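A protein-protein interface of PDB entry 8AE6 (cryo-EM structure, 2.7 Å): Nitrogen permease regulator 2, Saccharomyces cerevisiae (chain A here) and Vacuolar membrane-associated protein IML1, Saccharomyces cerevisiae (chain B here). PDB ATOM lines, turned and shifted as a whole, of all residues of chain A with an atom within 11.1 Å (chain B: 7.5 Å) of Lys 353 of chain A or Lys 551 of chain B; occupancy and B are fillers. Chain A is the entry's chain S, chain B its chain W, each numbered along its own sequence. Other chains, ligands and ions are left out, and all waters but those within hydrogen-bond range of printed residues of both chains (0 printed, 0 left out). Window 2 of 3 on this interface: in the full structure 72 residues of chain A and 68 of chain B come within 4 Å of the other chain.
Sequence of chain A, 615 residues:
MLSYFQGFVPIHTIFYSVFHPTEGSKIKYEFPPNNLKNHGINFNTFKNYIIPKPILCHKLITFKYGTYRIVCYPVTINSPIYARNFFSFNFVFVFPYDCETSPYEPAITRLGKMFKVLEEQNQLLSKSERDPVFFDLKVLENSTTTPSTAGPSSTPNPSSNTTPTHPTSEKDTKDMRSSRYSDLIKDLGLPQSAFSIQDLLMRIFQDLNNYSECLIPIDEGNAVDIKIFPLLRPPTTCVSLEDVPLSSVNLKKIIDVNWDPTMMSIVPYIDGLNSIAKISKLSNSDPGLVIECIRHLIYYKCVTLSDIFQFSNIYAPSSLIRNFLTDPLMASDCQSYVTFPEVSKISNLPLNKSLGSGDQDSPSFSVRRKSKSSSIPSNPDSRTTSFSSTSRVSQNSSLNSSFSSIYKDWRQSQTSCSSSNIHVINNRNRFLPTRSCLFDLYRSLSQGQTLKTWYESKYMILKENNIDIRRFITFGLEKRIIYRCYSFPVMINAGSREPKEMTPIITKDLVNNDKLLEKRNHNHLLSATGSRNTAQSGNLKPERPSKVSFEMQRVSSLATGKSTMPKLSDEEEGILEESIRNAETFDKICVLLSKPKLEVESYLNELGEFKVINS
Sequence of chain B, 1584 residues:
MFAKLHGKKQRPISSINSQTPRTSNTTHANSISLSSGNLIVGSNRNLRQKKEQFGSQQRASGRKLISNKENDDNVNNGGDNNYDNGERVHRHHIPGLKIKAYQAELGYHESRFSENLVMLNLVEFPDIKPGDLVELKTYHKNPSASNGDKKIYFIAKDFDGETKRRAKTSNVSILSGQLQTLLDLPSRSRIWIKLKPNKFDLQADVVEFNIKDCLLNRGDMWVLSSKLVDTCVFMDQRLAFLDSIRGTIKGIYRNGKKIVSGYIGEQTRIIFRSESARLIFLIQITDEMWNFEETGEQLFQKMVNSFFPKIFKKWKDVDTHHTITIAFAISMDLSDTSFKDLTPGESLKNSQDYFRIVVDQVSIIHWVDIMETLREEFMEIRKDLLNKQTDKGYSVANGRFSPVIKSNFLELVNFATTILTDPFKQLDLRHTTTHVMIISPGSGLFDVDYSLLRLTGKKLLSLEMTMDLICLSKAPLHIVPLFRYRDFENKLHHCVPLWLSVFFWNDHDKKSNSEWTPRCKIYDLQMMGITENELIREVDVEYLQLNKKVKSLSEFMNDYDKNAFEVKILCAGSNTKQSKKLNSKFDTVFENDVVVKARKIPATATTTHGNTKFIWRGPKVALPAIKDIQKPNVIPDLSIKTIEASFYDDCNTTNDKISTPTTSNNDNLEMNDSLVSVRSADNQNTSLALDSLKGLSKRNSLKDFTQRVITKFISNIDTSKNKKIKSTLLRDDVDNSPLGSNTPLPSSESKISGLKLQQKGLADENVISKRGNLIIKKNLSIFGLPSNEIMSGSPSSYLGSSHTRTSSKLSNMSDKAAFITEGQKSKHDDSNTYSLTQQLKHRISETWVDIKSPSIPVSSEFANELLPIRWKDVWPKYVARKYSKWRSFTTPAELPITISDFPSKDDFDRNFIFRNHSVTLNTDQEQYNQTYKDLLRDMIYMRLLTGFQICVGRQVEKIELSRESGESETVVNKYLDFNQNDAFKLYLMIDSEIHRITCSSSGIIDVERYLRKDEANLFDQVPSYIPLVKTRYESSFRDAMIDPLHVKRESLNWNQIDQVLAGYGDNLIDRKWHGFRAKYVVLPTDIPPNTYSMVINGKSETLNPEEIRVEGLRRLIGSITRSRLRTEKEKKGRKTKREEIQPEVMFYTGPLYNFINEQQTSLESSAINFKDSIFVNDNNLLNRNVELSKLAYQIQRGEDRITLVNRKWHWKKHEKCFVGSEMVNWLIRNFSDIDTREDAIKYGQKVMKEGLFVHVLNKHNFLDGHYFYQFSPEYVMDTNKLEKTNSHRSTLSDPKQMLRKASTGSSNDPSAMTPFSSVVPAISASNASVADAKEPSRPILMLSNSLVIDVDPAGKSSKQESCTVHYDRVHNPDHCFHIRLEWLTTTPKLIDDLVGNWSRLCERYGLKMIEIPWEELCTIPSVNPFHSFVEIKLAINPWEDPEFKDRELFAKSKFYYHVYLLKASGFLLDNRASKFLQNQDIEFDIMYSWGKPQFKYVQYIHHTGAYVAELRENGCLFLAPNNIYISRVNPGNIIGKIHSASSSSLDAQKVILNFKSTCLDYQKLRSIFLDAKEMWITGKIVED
Among the printed residues, pairs that only touch across the chains: Asn 352 of chain A with Ser 552 of chain B (3.3 Å), Pro 350 of chain A with Ser 552 of chain B (3.4 Å), Pro 350 of chain A with Lys 551 of chain B (3.4 Å), Leu 349 of chain A with Ser 552 of chain B (3.5 Å), Lys 353 of chain A with Lys 551 of chain B (3.7 Å), Ile 346 of chain A with Phe 556 of chain B (3.7 Å), Lys 345 of chain A with Leu 546 of chain B (3.7 Å), Lys 353 of chain A with Ser 552 of chain B (3.7 Å), Tyr 459 of chain A with Leu 553 of chain B (3.8 Å), Leu 349 of chain A with Leu 546 of chain B (3.8 Å), Leu 349 of chain A with Val 550 of chain B (3.8 Å), Ile 346 of chain A with Leu 546 of chain B (3.9 Å) and Ile 346 of chain A with Leu 553 of chain B (3.99 Å).
The side-chain hydroxyl (OG) of Ser 552 of chain B is in hydrogen-bond range of the backbone NH (N) of Ser 554 of chain B (3.1 Å).
Lys 551 of chain B touches just these residues of chain A: Pro 350 (3.4 Å) and Lys 353 (3.7 Å).
Val 550 of chain B touches one residue of chain A.
Of chain A, only Leu 349, Pro 350, Leu 351, Asn 352 and Lys 353 come within 4 Å of Ser 552 of chain B.
Printed residues of chain B within 4 Å of Tyr 459 of chain A: Leu 553 (3.8 Å).
Of the printed residues of chain B, Leu 349 of chain A touches Leu 546 (3.8 Å), Val 550 (3.8 Å) and Ser 552 (3.5 Å).
Printed residues of chain A within 4 Å of Ser 554 of chain B: Leu 351 and Asn 352.
Of the printed residues of chain B, Asn 352 of chain A touches Ser 552 (3.3 Å) and Ser 554 (3.2 Å).
Of the printed residues of chain B, Pro 350 of chain A touches Lys 551 (3.4 Å), Ser 552 (3.4 Å) and Leu 553 (2.6 Å).
The nearest residue of chain B that does not touch Lys 353 of chain A is Glu 555 of chain B (5.6 Å).
The nearest printed residue of chain B that does not touch Asn 352 of chain A is Leu 553 of chain B (4.8 Å).
OG of Ser 554 of chain B is in hydrogen-bond range of O of Leu 351 of chain A (2.8 Å).
O of Pro 350 of chain A is in hydrogen-bond range of N of Leu 553 of chain B.
OG of Ser 554 of chain B lies within hydrogen-bond range of OD1 of Asn 352 of chain A (3.2 Å).
O of Leu 351 of chain A is in hydrogen-bond range of N of Leu 553 of chain B (3.4 Å).
The backbone carbonyl oxygen (O) of Leu 351 of chain A lies within hydrogen-bond range of the side-chain hydroxyl (OG) of Ser 552 of chain B (2.4 Å).
Hydrophobic or aromatic side chains of chain B that line the printed part of chain A: Leu 546, Val 550, Leu 553 and Phe 556.
Along chain B the printed residues that touch a printed residue of chain A span positions 546 to 556.
Among the printed residues, no Asp or Glu carboxylate lies within 4 Å of a Lys or Arg side-chain nitrogen of the other chain.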
ATOM      1  N   LYS A 345      26.538  16.537  11.140  1.00  0.00           N
ATOM      2  CA  LYS A 345      26.549  16.218   9.722  1.00  0.00           C
ATOM      3  C   LYS A 345      25.428  16.907   8.958  1.00  0.00           C
ATOM      4  O   LYS A 345      25.569  17.117   7.748  1.00  0.00           O
ATOM      5  CB  LYS A 345      26.464  14.706   9.526  1.00  0.00           C
ATOM      6  CG  LYS A 345      27.680  13.955  10.034  1.00  0.00           C
ATOM      7  CD  LYS A 345      27.346  13.128  11.263  1.00  0.00           C
ATOM      8  CE  LYS A 345      28.559  12.355  11.754  1.00  0.00           C
ATOM      9  NZ  LYS A 345      28.265  11.592  13.000  1.00  0.00           N
ATOM     10  N   ILE A 346      24.330  17.266   9.632  1.00  0.00           N
ATOM     11  CA  ILE A 346      23.256  18.029   8.997  1.00  0.00           C
ATOM     12  C   ILE A 346      23.760  19.398   8.569  1.00  0.00           C
ATOM     13  O   ILE A 346      23.365  19.920   7.517  1.00  0.00           O
ATOM     14  CB  ILE A 346      22.043  18.123   9.946  1.00  0.00           C
ATOM     15  CG1 ILE A 346      21.527  16.721  10.274  1.00  0.00           C
ATOM     16  CG2 ILE A 346      20.930  18.980   9.348  1.00  0.00           C
ATOM     17  CD1 ILE A 346      20.152  16.693  10.903  1.00  0.00           C
ATOM     18  N   SER A 347      24.688  19.972   9.326  1.00  0.00           N
ATOM     19  CA  SER A 347      25.359  21.210   8.953  1.00  0.00           C
ATOM     20  C   SER A 347      26.430  21.009   7.876  1.00  0.00           C
ATOM     21  O   SER A 347      27.272  21.894   7.688  1.00  0.00           O
ATOM     22  CB  SER A 347      25.977  21.863  10.188  1.00  0.00           C
ATOM     23  OG  SER A 347      26.951  22.824   9.826  1.00  0.00           O
ATOM     24  N   ASN A 348      26.441  19.860   7.198  1.00  0.00           N
ATOM     25  CA  ASN A 348      27.257  19.644   6.018  1.00  0.00           C
ATOM     26  C   ASN A 348      26.446  19.220   4.800  1.00  0.00           C
ATOM     27  O   ASN A 348      26.975  19.266   3.684  1.00  0.00           O
ATOM     28  CB  ASN A 348      28.333  18.582   6.292  1.00  0.00           C
ATOM     29  CG  ASN A 348      29.230  18.949   7.457  1.00  0.00           C
ATOM     30  OD1 ASN A 348      29.565  20.115   7.653  1.00  0.00           O
ATOM     31  ND2 ASN A 348      29.623  17.950   8.238  1.00  0.00           N
ATOM     32  N   LEU A 349      25.196  18.807   4.984  1.00  0.00           N
ATOM     33  CA  LEU A 349      24.363  18.393   3.859  1.00  0.00           C
ATOM     34  C   LEU A 349      23.957  19.595   3.016  1.00  0.00           C
ATOM     35  O   LEU A 349      23.579  20.636   3.567  1.00  0.00           O
ATOM     36  CB  LEU A 349      23.115  17.669   4.356  1.00  0.00           C
ATOM     37  CG  LEU A 349      23.088  16.140   4.362  1.00  0.00           C
ATOM     38  CD1 LEU A 349      24.089  15.557   5.331  1.00  0.00           C
ATOM     39  CD2 LEU A 349      21.690  15.660   4.703  1.00  0.00           C
ATOM     40  N   PRO A 350      24.019  19.498   1.692  1.00  0.00           N
ATOM     41  CA  PRO A 350      23.436  20.533   0.838  1.00  0.00           C
ATOM     42  C   PRO A 350      21.922  20.388   0.778  1.00  0.00           C
ATOM     43  O   PRO A 350      21.346  19.386   1.207  1.00  0.00           O
ATOM     44  CB  PRO A 350      24.075  20.264  -0.524  1.00  0.00           C
ATOM     45  CG  PRO A 350      24.346  18.806  -0.515  1.00  0.00           C
ATOM     46  CD  PRO A 350      24.654  18.425   0.908  1.00  0.00           C
ATOM     47  N   LEU A 351      21.276  21.424   0.241  1.00  0.00           N
ATOM     48  CA  LEU A 351      19.821  21.409   0.131  1.00  0.00           C
ATOM     49  C   LEU A 351      19.350  20.377  -0.884  1.00  0.00           C
ATOM     50  O   LEU A 351      18.378  19.654  -0.638  1.00  0.00           O
ATOM     51  CB  LEU A 351      19.307  22.801  -0.240  1.00  0.00           C
ATOM     52  CG  LEU A 351      17.788  22.982  -0.221  1.00  0.00           C
ATOM     53  CD1 LEU A 351      17.272  22.946   1.202  1.00  0.00           C
ATOM     54  CD2 LEU A 351      17.394  24.277  -0.901  1.00  0.00           C
ATOM     55  N   ASN A 352      20.024  20.291  -2.028  1.00  0.00           N
ATOM     56  CA  ASN A 352      19.669  19.337  -3.068  1.00  0.00           C
ATOM     57  C   ASN A 352      20.931  18.697  -3.620  1.00  0.00           C
ATOM     58  O   ASN A 352      21.953  19.367  -3.786  1.00  0.00           O
ATOM     59  CB  ASN A 352      18.880  20.009  -4.196  1.00  0.00           C
ATOM     60  CG  ASN A 352      17.389  19.979  -3.958  1.00  0.00           C
ATOM     61  OD1 ASN A 352      16.852  19.005  -3.431  1.00  0.00           O
ATOM     62  ND2 ASN A 352      16.706  21.051  -4.342  1.00  0.00           N
ATOM     63  N   LYS A 353      20.850  17.403  -3.904  1.00  0.00           N
ATOM     64  CA  LYS A 353      21.977  16.666  -4.459  1.00  0.00           C
ATOM     65  C   LYS A 353      21.493  15.458  -5.253  1.00  0.00           C
ATOM     66  O   LYS A 353      20.764  14.616  -4.734  1.00  0.00           O
ATOM     67  CB  LYS A 353      22.930  16.222  -3.350  1.00  0.00           C
ATOM     68  CG  LYS A 353      24.186  15.531  -3.853  1.00  0.00           C
ATOM     69  CD  LYS A 353      25.184  15.313  -2.728  1.00  0.00           C
ATOM     70  CE  LYS A 353      26.484  14.722  -3.252  1.00  0.00           C
ATOM     71  NZ  LYS A 353      27.492  14.554  -2.170  1.00  0.00           N
ATOM     72  N   TYR A 459      18.472  28.020   4.950  1.00  0.00           N
ATOM     73  CA  TYR A 459      19.263  26.857   5.315  1.00  0.00           C
ATOM     74  C   TYR A 459      20.743  27.148   5.462  1.00  0.00           C
ATOM     75  O   TYR A 459      21.417  26.421   6.193  1.00  0.00           O
ATOM     76  CB  TYR A 459      19.074  25.718   4.299  1.00  0.00           C
ATOM     77  CG  TYR A 459      19.825  25.867   2.997  1.00  0.00           C
ATOM     78  CD1 TYR A 459      19.439  26.808   2.054  1.00  0.00           C
ATOM     79  CD2 TYR A 459      20.901  25.043   2.697  1.00  0.00           C
ATOM     80  CE1 TYR A 459      20.115  26.941   0.859  1.00  0.00           C
ATOM     81  CE2 TYR A 459      21.585  25.166   1.506  1.00  0.00           C
ATOM     82  CZ  TYR A 459      21.186  26.117   0.591  1.00  0.00           C
ATOM     83  OH  TYR A 459      21.865  26.244  -0.600  1.00  0.00           O
ATOM     84  N   LYS A 463      22.785  26.245   8.851  1.00  0.00           N
ATOM     85  CA  LYS A 463      23.983  25.431   8.656  1.00  0.00           C
ATOM     86  C   LYS A 463      25.223  26.124   9.205  1.00  0.00           C
ATOM     87  O   LYS A 463      26.061  25.485   9.850  1.00  0.00           O
ATOM     88  CB  LYS A 463      24.155  25.108   7.172  1.00  0.00           C
ATOM     89  CG  LYS A 463      25.423  24.371   6.822  1.00  0.00           C
ATOM     90  CD  LYS A 463      25.389  23.867   5.388  1.00  0.00           C
ATOM     91  CE  LYS A 463      25.562  25.005   4.398  1.00  0.00           C
ATOM     92  NZ  LYS A 463      25.655  24.512   2.995  1.00  0.00           N
ATOM     93  N   LEU B 546      21.118  11.481  11.975  1.00  0.00           N
ATOM     94  CA  LEU B 546      20.945  11.224  10.553  1.00  0.00           C
ATOM     95  C   LEU B 546      20.640   9.746  10.306  1.00  0.00           C
ATOM     96  O   LEU B 546      20.362   8.976  11.229  1.00  0.00           O
ATOM     97  CB  LEU B 546      22.180  11.665   9.774  1.00  0.00           C
ATOM     98  CG  LEU B 546      22.139  13.053   9.138  1.00  0.00           C
ATOM     99  CD1 LEU B 546      23.327  13.239   8.221  1.00  0.00           C
ATOM    100  CD2 LEU B 546      20.844  13.254   8.377  1.00  0.00           C
ATOM    101  N   LYS B 548      22.586   7.951   7.600  1.00  0.00           N
ATOM    102  CA  LYS B 548      23.706   7.418   6.804  1.00  0.00           C
ATOM    103  C   LYS B 548      23.217   6.846   5.473  1.00  0.00           C
ATOM    104  O   LYS B 548      23.790   5.902   4.927  1.00  0.00           O
ATOM    105  CB  LYS B 548      24.529   6.385   7.584  1.00  0.00           C
ATOM    106  CG  LYS B 548      26.019   6.420   7.273  1.00  0.00           C
ATOM    107  CD  LYS B 548      26.763   5.300   7.975  1.00  0.00           C
ATOM    108  CE  LYS B 548      28.241   5.312   7.616  1.00  0.00           C
ATOM    109  NZ  LYS B 548      28.973   4.163   8.215  1.00  0.00           N
ATOM    110  N   LYS B 549      22.141   7.429   4.952  1.00  0.00           N
ATOM    111  CA  LYS B 549      21.642   7.124   3.622  1.00  0.00           C
ATOM    112  C   LYS B 549      21.135   8.367   2.910  1.00  0.00           C
ATOM    113  O   LYS B 549      20.548   8.243   1.832  1.00  0.00           O
ATOM    114  CB  LYS B 549      20.514   6.082   3.692  1.00  0.00           C
ATOM    115  CG  LYS B 549      20.934   4.672   3.309  1.00  0.00           C
ATOM    116  CD  LYS B 549      19.880   3.658   3.722  1.00  0.00           C
ATOM    117  CE  LYS B 549      20.303   2.241   3.372  1.00  0.00           C
ATOM    118  NZ  LYS B 549      19.283   1.239   3.787  1.00  0.00           N
ATOM    119  N   VAL B 550      21.340   9.548   3.482  1.00  0.00           N
ATOM    120  CA  VAL B 550      20.716  10.784   3.030  1.00  0.00           C
ATOM    121  C   VAL B 550      21.821  11.761   2.662  1.00  0.00           C
ATOM    122  O   VAL B 550      22.701  12.050   3.480  1.00  0.00           O
ATOM    123  CB  VAL B 550      19.799  11.366   4.115  1.00  0.00           C
ATOM    124  CG1 VAL B 550      19.378  12.760   3.764  1.00  0.00           C
ATOM    125  CG2 VAL B 550      18.580  10.479   4.309  1.00  0.00           C
ATOM    126  N   LYS B 551      21.777  12.273   1.432  1.00  0.00           N
ATOM    127  CA  LYS B 551      22.794  13.182   0.925  1.00  0.00           C
ATOM    128  C   LYS B 551      22.275  14.589   0.676  1.00  0.00           C
ATOM    129  O   LYS B 551      23.052  15.455   0.265  1.00  0.00           O
ATOM    130  CB  LYS B 551      23.401  12.625  -0.368  1.00  0.00           C
ATOM    131  CG  LYS B 551      23.630  11.123  -0.358  1.00  0.00           C
ATOM    132  CD  LYS B 551      24.707  10.729   0.641  1.00  0.00           C
ATOM    133  CE  LYS B 551      24.748   9.223   0.844  1.00  0.00           C
ATOM    134  NZ  LYS B 551      25.752   8.827   1.869  1.00  0.00           N
ATOM    135  N   SER B 552      20.992  14.844   0.909  1.00  0.00           N
ATOM    136  CA  SER B 552      20.403  16.151   0.659  1.00  0.00           C
ATOM    137  C   SER B 552      19.528  16.547   1.836  1.00  0.00           C
ATOM    138  O   SER B 552      18.980  15.699   2.536  1.00  0.00           O
ATOM    139  CB  SER B 552      19.575  16.157  -0.627  1.00  0.00           C
ATOM    140  OG  SER B 552      18.686  17.259  -0.651  1.00  0.00           O
ATOM    141  N   LEU B 553      19.395  17.857   2.039  1.00  0.00           N
ATOM    142  CA  LEU B 553      18.553  18.354   3.121  1.00  0.00           C
ATOM    143  C   LEU B 553      17.077  18.119   2.818  1.00  0.00           C
ATOM    144  O   LEU B 553      16.288  17.814   3.724  1.00  0.00           O
ATOM    145  CB  LEU B 553      18.842  19.835   3.344  1.00  0.00           C
ATOM    146  CG  LEU B 553      18.548  20.473   4.693  1.00  0.00           C
ATOM    147  CD1 LEU B 553      19.390  19.823   5.769  1.00  0.00           C
ATOM    148  CD2 LEU B 553      18.847  21.956   4.611  1.00  0.00           C
ATOM    149  N   SER B 554      16.694  18.243   1.544  1.00  0.00           N
ATOM    150  CA  SER B 554      15.328  17.938   1.133  1.00  0.00           C
ATOM    151  C   SER B 554      15.015  16.459   1.308  1.00  0.00           C
ATOM    152  O   SER B 554      13.899  16.096   1.702  1.00  0.00           O
ATOM    153  CB  SER B 554      15.111  18.366  -0.314  1.00  0.00           C
ATOM    154  OG  SER B 554      15.595  19.677  -0.536  1.00  0.00           O
ATOM    155  N   GLU B 555      15.987  15.590   1.014  1.00  0.00           N
ATOM    156  CA  GLU B 555      15.810  14.163   1.262  1.00  0.00           C
ATOM    157  C   GLU B 555      15.682  13.864   2.747  1.00  0.00           C
ATOM    158  O   GLU B 555      14.918  12.972   3.131  1.00  0.00           O
ATOM    159  CB  GLU B 555      16.972  13.376   0.659  1.00  0.00           C
ATOM    160  CG  GLU B 555      16.992  13.364  -0.858  1.00  0.00           C
ATOM    161  CD  GLU B 555      15.838  12.581  -1.451  1.00  0.00           C
ATOM    162  OE1 GLU B 555      15.464  11.539  -0.871  1.00  0.00           O
ATOM    163  OE2 GLU B 555      15.306  13.004  -2.498  1.00  0.00           O
ATOM    164  N   PHE B 556      16.409  14.601   3.592  1.00  0.00           N
ATOM    165  CA  PHE B 556      16.266  14.448   5.034  1.00  0.00           C
ATOM    166  C   PHE B 556      14.874  14.849   5.501  1.00  0.00           C
ATOM    167  O   PHE B 556      14.266  14.157   6.327  1.00  0.00           O
ATOM    168  CB  PHE B 556      17.326  15.278   5.757  1.00  0.00           C
ATOM    169  CG  PHE B 556      17.148  15.324   7.245  1.00  0.00           C
ATOM    170  CD1 PHE B 556      17.346  14.194   8.014  1.00  0.00           C
ATOM    171  CD2 PHE B 556      16.778  16.500   7.873  1.00  0.00           C
ATOM    172  CE1 PHE B 556      17.184  14.235   9.383  1.00  0.00           C
ATOM    173  CE2 PHE B 556      16.612  16.543   9.240  1.00  0.00           C
ATOM    174  CZ  PHE B 556      16.816  15.411   9.995  1.00  0.00           C
ATOM    175  N   ASP B 559      12.419  12.111   4.313  1.00  0.00           N
ATOM    176  CA  ASP B 559      12.521  10.891   5.102  1.00  0.00           C
ATOM    177  C   ASP B 559      12.034  11.096   6.529  1.00  0.00           C
ATOM    178  O   ASP B 559      11.567  10.144   7.163  1.00  0.00           O
ATOM    179  CB  ASP B 559      13.960  10.377   5.105  1.00  0.00           C
ATOM    180  CG  ASP B 559      14.285   9.553   3.877  1.00  0.00           C
ATOM    181  OD1 ASP B 559      13.360   8.933   3.316  1.00  0.00           O
ATOM    182  OD2 ASP B 559      15.467   9.528   3.473  1.00  0.00           O
